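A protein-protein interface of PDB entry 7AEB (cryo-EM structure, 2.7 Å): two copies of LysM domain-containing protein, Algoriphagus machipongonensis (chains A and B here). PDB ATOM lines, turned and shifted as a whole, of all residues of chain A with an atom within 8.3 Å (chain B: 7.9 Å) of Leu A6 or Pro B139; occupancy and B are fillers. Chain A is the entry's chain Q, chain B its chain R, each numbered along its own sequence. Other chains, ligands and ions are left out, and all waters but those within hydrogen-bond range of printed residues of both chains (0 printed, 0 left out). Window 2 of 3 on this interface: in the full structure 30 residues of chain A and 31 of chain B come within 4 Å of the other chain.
The backbone carbonyl oxygen of Glu A7 sits at hydrogen-bond distance from the side-chain amide nitrogen of Asn A33, at 2.9 Å.
OD1 of Asp B140 sits at hydrogen-bond distance from OG1 of Thr B142 (3.3 Å).
OE2 of Glu A7 lies within salt-bridge range of NZ of Lys A5, at 3.5 Å.
O of Glu A7 sits at hydrogen-bond distance from NE1 of Trp A118 (3.4 Å).
Pro B139 touches just these residues of chain A: Lys A5, Leu A6 and Glu A7.
Of the printed residues of chain B, Glu A7 touches Pro B139.
Printed residues of chain B within 4 Å of Lys A5: Pro B139 (3.2 Å) and Asp B140 (3.8 Å).
Printed residues of chain A within 4 Å of Asp B140: Lys A5 (3.8 Å) and Gly A119 (3.7 Å).
Printed residues of chain A within 4 Å of Gly B141: Gly A119 (3.6 Å).
Leu A9 touches none of the printed residues of chain B.
The nearest residue of chain B that does not touch Leu A6 is Asp B140 (5.1 Å).
O of Lys A5 sits close to O of Pro B139 (3.2 Å).
N of Glu A7 lies within hydrogen-bond range of O of Pro B139 (3.0 Å).
Lys A5 touches Asp B140.
O of Pro B139 touches CA of Leu A6, 3.2 Å away.
CA of Gly A119 touches O of Asp B140, 3.7 Å away.
CA of Gly A119 touches O of Gly B141, at 3.6 Å.
No position is printed for both chains.
Of the 6 pairs that touch across the chains among the printed residues, none has its exchanged pair printed and touching as well.
Of the 14 printed residues of chain A, 4 touch a printed residue of chain B.
Hydrophobic or aromatic side chains of chain A that line the printed part of chain B: Leu A6.
Among the printed residues, no Asp or Glu carboxylate lies within 4 Å of a Lys or Arg side-chain nitrogen of the other chain.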
ATOM      1  N   SER A   2      29.305   4.272  14.422  1.00  0.00           N
ATOM      2  CA  SER A   2      29.417   3.560  15.687  1.00  0.00           C
ATOM      3  C   SER A   2      28.681   4.293  16.798  1.00  0.00           C
ATOM      4  O   SER A   2      28.971   4.098  17.973  1.00  0.00           O
ATOM      5  CB  SER A   2      30.887   3.371  16.065  1.00  0.00           C
ATOM      6  OG  SER A   2      31.022   3.048  17.437  1.00  0.00           O
ATOM      7  N   GLU A   3      27.761   5.166  16.394  1.00  0.00           N
ATOM      8  CA  GLU A   3      26.841   5.806  17.321  1.00  0.00           C
ATOM      9  C   GLU A   3      25.881   4.785  17.904  1.00  0.00           C
ATOM     10  O   GLU A   3      25.536   4.839  19.092  1.00  0.00           O
ATOM     11  CB  GLU A   3      26.049   6.903  16.607  1.00  0.00           C
ATOM     12  CG  GLU A   3      25.138   7.698  17.519  1.00  0.00           C
ATOM     13  CD  GLU A   3      24.403   8.812  16.799  1.00  0.00           C
ATOM     14  OE1 GLU A   3      23.490   9.415  17.400  1.00  0.00           O
ATOM     15  OE2 GLU A   3      24.678   9.019  15.598  1.00  0.00           O
ATOM     16  N   GLY A   4      25.445   3.846  17.065  1.00  0.00           N
ATOM     17  CA  GLY A   4      24.468   2.844  17.420  1.00  0.00           C
ATOM     18  C   GLY A   4      24.972   1.751  18.325  1.00  0.00           C
ATOM     19  O   GLY A   4      24.182   0.905  18.748  1.00  0.00           O
ATOM     20  N   LYS A   5      26.263   1.746  18.634  1.00  0.00           N
ATOM     21  CA  LYS A   5      26.840   0.750  19.522  1.00  0.00           C
ATOM     22  C   LYS A   5      26.584   1.105  20.976  1.00  0.00           C
ATOM     23  O   LYS A   5      26.844   2.231  21.403  1.00  0.00           O
ATOM     24  CB  LYS A   5      28.343   0.640  19.276  1.00  0.00           C
ATOM     25  CG  LYS A   5      29.035  -0.333  20.196  1.00  0.00           C
ATOM     26  CD  LYS A   5      30.524  -0.123  20.224  1.00  0.00           C
ATOM     27  CE  LYS A   5      31.165  -1.020  21.258  1.00  0.00           C
ATOM     28  NZ  LYS A   5      32.647  -0.921  21.232  1.00  0.00           N
ATOM     29  N   LEU A   6      26.088   0.133  21.741  1.00  0.00           N
ATOM     30  CA  LEU A   6      25.954   0.255  23.189  1.00  0.00           C
ATOM     31  C   LEU A   6      27.316   0.018  23.829  1.00  0.00           C
ATOM     32  O   LEU A   6      27.809  -1.112  23.863  1.00  0.00           O
ATOM     33  CB  LEU A   6      24.919  -0.733  23.719  1.00  0.00           C
ATOM     34  CG  LEU A   6      24.592  -0.664  25.216  1.00  0.00           C
ATOM     35  CD1 LEU A   6      23.937   0.645  25.573  1.00  0.00           C
ATOM     36  CD2 LEU A   6      23.707  -1.815  25.635  1.00  0.00           C
ATOM     37  N   GLU A   7      27.925   1.079  24.348  1.00  0.00           N
ATOM     38  CA  GLU A   7      29.225   0.968  24.989  1.00  0.00           C
ATOM     39  C   GLU A   7      29.087   0.408  26.403  1.00  0.00           C
ATOM     40  O   GLU A   7      28.110   0.678  27.103  1.00  0.00           O
ATOM     41  CB  GLU A   7      29.908   2.339  25.020  1.00  0.00           C
ATOM     42  CG  GLU A   7      31.377   2.322  25.422  1.00  0.00           C
ATOM     43  CD  GLU A   7      32.308   1.882  24.301  1.00  0.00           C
ATOM     44  OE1 GLU A   7      33.465   1.531  24.592  1.00  0.00           O
ATOM     45  OE2 GLU A   7      31.891   1.894  23.125  1.00  0.00           O
ATOM     46  N   LYS A   8      30.072  -0.386  26.815  1.00  0.00           N
ATOM     47  CA  LYS A   8      30.099  -1.029  28.119  1.00  0.00           C
ATOM     48  C   LYS A   8      31.226  -0.454  28.968  1.00  0.00           C
ATOM     49  O   LYS A   8      32.280  -0.084  28.447  1.00  0.00           O
ATOM     50  CB  LYS A   8      30.272  -2.537  27.960  1.00  0.00           C
ATOM     51  CG  LYS A   8      29.037  -3.229  27.438  1.00  0.00           C
ATOM     52  CD  LYS A   8      27.981  -3.322  28.513  1.00  0.00           C
ATOM     53  CE  LYS A   8      26.618  -3.553  27.924  1.00  0.00           C
ATOM     54  NZ  LYS A   8      26.596  -4.743  27.048  1.00  0.00           N
ATOM     55  N   LEU A   9      30.998  -0.387  30.277  1.00  0.00           N
ATOM     56  CA  LEU A   9      31.943   0.231  31.201  1.00  0.00           C
ATOM     57  C   LEU A   9      33.168  -0.663  31.405  1.00  0.00           C
ATOM     58  O   LEU A   9      33.060  -1.888  31.434  1.00  0.00           O
ATOM     59  CB  LEU A   9      31.227   0.521  32.523  1.00  0.00           C
ATOM     60  CG  LEU A   9      31.895   0.827  33.867  1.00  0.00           C
ATOM     61  CD1 LEU A   9      32.834   1.971  33.769  1.00  0.00           C
ATOM     62  CD2 LEU A   9      30.851   1.163  34.885  1.00  0.00           C
ATOM     63  N   LEU A  31      29.307  -6.786  31.833  1.00  0.00           N
ATOM     64  CA  LEU A  31      28.323  -7.289  30.886  1.00  0.00           C
ATOM     65  C   LEU A  31      26.998  -6.546  30.959  1.00  0.00           C
ATOM     66  O   LEU A  31      26.225  -6.592  30.001  1.00  0.00           O
ATOM     67  CB  LEU A  31      28.075  -8.784  31.105  1.00  0.00           C
ATOM     68  CG  LEU A  31      29.279  -9.729  31.007  1.00  0.00           C
ATOM     69  CD1 LEU A  31      29.017 -10.982  31.804  1.00  0.00           C
ATOM     70  CD2 LEU A  31      29.611 -10.086  29.574  1.00  0.00           C
ATOM     71  N   LEU A  32      26.715  -5.884  32.078  1.00  0.00           N
ATOM     72  CA  LEU A  32      25.565  -5.003  32.214  1.00  0.00           C
ATOM     73  C   LEU A  32      26.013  -3.709  32.867  1.00  0.00           C
ATOM     74  O   LEU A  32      26.701  -3.727  33.886  1.00  0.00           O
ATOM     75  CB  LEU A  32      24.451  -5.644  33.038  1.00  0.00           C
ATOM     76  CG  LEU A  32      23.818  -6.924  32.498  1.00  0.00           C
ATOM     77  CD1 LEU A  32      23.241  -7.731  33.638  1.00  0.00           C
ATOM     78  CD2 LEU A  32      22.757  -6.604  31.467  1.00  0.00           C
ATOM     79  N   ASN A  33      25.620  -2.611  32.280  1.00  0.00           N
ATOM     80  CA  ASN A  33      25.945  -1.268  32.729  1.00  0.00           C
ATOM     81  C   ASN A  33      25.168  -0.914  33.994  1.00  0.00           C
ATOM     82  O   ASN A  33      24.053  -1.399  34.195  1.00  0.00           O
ATOM     83  CB  ASN A  33      25.602  -0.256  31.636  1.00  0.00           C
ATOM     84  CG  ASN A  33      26.718  -0.075  30.639  1.00  0.00           C
ATOM     85  OD1 ASN A  33      27.875   0.010  31.011  1.00  0.00           O
ATOM     86  ND2 ASN A  33      26.373  -0.019  29.365  1.00  0.00           N
ATOM     87  N   TYR A  83      24.824 -13.452  25.176  1.00  0.00           N
ATOM     88  CA  TYR A  83      25.735 -14.146  26.068  1.00  0.00           C
ATOM     89  C   TYR A  83      25.341 -15.610  26.194  1.00  0.00           C
ATOM     90  O   TYR A  83      24.222 -16.002  25.863  1.00  0.00           O
ATOM     91  CB  TYR A  83      25.756 -13.488  27.448  1.00  0.00           C
ATOM     92  CG  TYR A  83      26.167 -12.047  27.383  1.00  0.00           C
ATOM     93  CD1 TYR A  83      27.274 -11.666  26.641  1.00  0.00           C
ATOM     94  CD2 TYR A  83      25.444 -11.062  28.041  1.00  0.00           C
ATOM     95  CE1 TYR A  83      27.659 -10.343  26.557  1.00  0.00           C
ATOM     96  CE2 TYR A  83      25.821  -9.732  27.970  1.00  0.00           C
ATOM     97  CZ  TYR A  83      26.932  -9.379  27.226  1.00  0.00           C
ATOM     98  OH  TYR A  83      27.324  -8.064  27.142  1.00  0.00           O
ATOM     99  N   TRP A 118      33.720   5.197  30.891  1.00  0.00           N
ATOM    100  CA  TRP A 118      32.473   4.838  30.219  1.00  0.00           C
ATOM    101  C   TRP A 118      31.912   6.089  29.564  1.00  0.00           C
ATOM    102  O   TRP A 118      31.384   6.957  30.260  1.00  0.00           O
ATOM    103  CB  TRP A 118      31.466   4.245  31.195  1.00  0.00           C
ATOM    104  CG  TRP A 118      30.128   3.932  30.590  1.00  0.00           C
ATOM    105  CD1 TRP A 118      29.884   3.457  29.340  1.00  0.00           C
ATOM    106  CD2 TRP A 118      28.855   4.060  31.223  1.00  0.00           C
ATOM    107  NE1 TRP A 118      28.542   3.297  29.148  1.00  0.00           N
ATOM    108  CE2 TRP A 118      27.886   3.659  30.290  1.00  0.00           C
ATOM    109  CE3 TRP A 118      28.438   4.482  32.489  1.00  0.00           C
ATOM    110  CZ2 TRP A 118      26.525   3.667  30.577  1.00  0.00           C
ATOM    111  CZ3 TRP A 118      27.088   4.484  32.775  1.00  0.00           C
ATOM    112  CH2 TRP A 118      26.147   4.078  31.823  1.00  0.00           C
ATOM    113  N   GLY A 119      32.001   6.166  28.241  1.00  0.00           N
ATOM    114  CA  GLY A 119      31.472   7.308  27.520  1.00  0.00           C
ATOM    115  C   GLY A 119      32.251   8.573  27.808  1.00  0.00           C
ATOM    116  O   GLY A 119      33.438   8.685  27.498  1.00  0.00           O
ATOM    117  N   LEU B 136      20.026   9.706  32.753  1.00  0.00           N
ATOM    118  CA  LEU B 136      19.815   9.107  31.438  1.00  0.00           C
ATOM    119  C   LEU B 136      21.049   9.247  30.565  1.00  0.00           C
ATOM    120  O   LEU B 136      21.818  10.199  30.696  1.00  0.00           O
ATOM    121  CB  LEU B 136      18.648   9.729  30.667  1.00  0.00           C
ATOM    122  CG  LEU B 136      17.184   9.351  30.775  1.00  0.00           C
ATOM    123  CD1 LEU B 136      16.446  10.219  29.796  1.00  0.00           C
ATOM    124  CD2 LEU B 136      16.982   7.903  30.422  1.00  0.00           C
ATOM    125  N   PHE B 137      21.206   8.296  29.646  1.00  0.00           N
ATOM    126  CA  PHE B 137      22.360   8.217  28.767  1.00  0.00           C
ATOM    127  C   PHE B 137      21.924   7.830  27.363  1.00  0.00           C
ATOM    128  O   PHE B 137      20.949   7.106  27.171  1.00  0.00           O
ATOM    129  CB  PHE B 137      23.401   7.198  29.276  1.00  0.00           C
ATOM    130  CG  PHE B 137      23.820   7.417  30.699  1.00  0.00           C
ATOM    131  CD1 PHE B 137      23.168   6.770  31.741  1.00  0.00           C
ATOM    132  CD2 PHE B 137      24.862   8.271  30.998  1.00  0.00           C
ATOM    133  CE1 PHE B 137      23.539   6.989  33.043  1.00  0.00           C
ATOM    134  CE2 PHE B 137      25.237   8.486  32.299  1.00  0.00           C
ATOM    135  CZ  PHE B 137      24.577   7.846  33.318  1.00  0.00           C
ATOM    136  N   ARG B 138      22.667   8.327  26.384  1.00  0.00           N
ATOM    137  CA  ARG B 138      22.626   7.814  25.023  1.00  0.00           C
ATOM    138  C   ARG B 138      23.333   6.458  24.975  1.00  0.00           C
ATOM    139  O   ARG B 138      24.093   6.134  25.887  1.00  0.00           O
ATOM    140  CB  ARG B 138      23.285   8.825  24.089  1.00  0.00           C
ATOM    141  CG  ARG B 138      22.347   9.860  23.525  1.00  0.00           C
ATOM    142  CD  ARG B 138      23.102  10.737  22.570  1.00  0.00           C
ATOM    143  NE  ARG B 138      22.536  12.075  22.479  1.00  0.00           N
ATOM    144  CZ  ARG B 138      23.224  13.149  22.106  1.00  0.00           C
ATOM    145  NH1 ARG B 138      24.508  13.040  21.791  1.00  0.00           N
ATOM    146  NH2 ARG B 138      22.631  14.328  22.048  1.00  0.00           N
ATOM    147  N   PRO B 139      23.066   5.629  23.938  1.00  0.00           N
ATOM    148  CA  PRO B 139      23.720   4.305  23.847  1.00  0.00           C
ATOM    149  C   PRO B 139      25.242   4.293  23.857  1.00  0.00           C
ATOM    150  O   PRO B 139      25.833   3.295  24.287  1.00  0.00           O
ATOM    151  CB  PRO B 139      23.193   3.760  22.515  1.00  0.00           C
ATOM    152  CG  PRO B 139      21.887   4.365  22.362  1.00  0.00           C
ATOM    153  CD  PRO B 139      21.933   5.712  22.994  1.00  0.00           C
ATOM    154  N   ASP B 140      25.896   5.369  23.434  1.00  0.00           N
ATOM    155  CA  ASP B 140      27.351   5.443  23.457  1.00  0.00           C
ATOM    156  C   ASP B 140      27.878   6.055  24.750  1.00  0.00           C
ATOM    157  O   ASP B 140      29.075   6.321  24.863  1.00  0.00           O
ATOM    158  CB  ASP B 140      27.873   6.212  22.244  1.00  0.00           C
ATOM    159  CG  ASP B 140      27.412   7.642  22.215  1.00  0.00           C
ATOM    160  OD1 ASP B 140      26.299   7.918  22.689  1.00  0.00           O
ATOM    161  OD2 ASP B 140      28.158   8.490  21.693  1.00  0.00           O
ATOM    162  N   GLY B 141      27.009   6.281  25.729  1.00  0.00           N
ATOM    163  CA  GLY B 141      27.420   6.765  27.029  1.00  0.00           C
ATOM    164  C   GLY B 141      27.445   8.265  27.193  1.00  0.00           C
ATOM    165  O   GLY B 141      28.168   8.758  28.061  1.00  0.00           O
ATOM    166  N   THR B 142      26.700   9.002  26.394  1.00  0.00           N
ATOM    167  CA  THR B 142      26.608  10.446  26.564  1.00  0.00           C
ATOM    168  C   THR B 142      25.433  10.781  27.476  1.00  0.00           C
ATOM    169  O   THR B 142      24.309  10.365  27.193  1.00  0.00           O
ATOM    170  CB  THR B 142      26.426  11.125  25.215  1.00  0.00           C
ATOM    171  OG1 THR B 142      27.361  10.579  24.282  1.00  0.00           O
ATOM    172  CG2 THR B 142      26.649  12.611  25.325  1.00  0.00           C
ATOM    173  N   ILE B 144      22.335  12.792  29.251  1.00  0.00           N
ATOM    174  CA  ILE B 144      21.351  13.763  28.791  1.00  0.00           C
ATOM    175  C   ILE B 144      20.454  14.259  29.917  1.00  0.00           C
ATOM    176  O   ILE B 144      19.585  15.103  29.679  1.00  0.00           O
ATOM    177  CB  ILE B 144      20.505  13.190  27.632  1.00  0.00           C
ATOM    178  CG1 ILE B 144      20.040  11.771  27.942  1.00  0.00           C
ATOM    179  CG2 ILE B 144      21.276  13.216  26.327  1.00  0.00           C
ATOM    180  CD1 ILE B 144      19.127  11.196  26.906  1.00  0.00           C
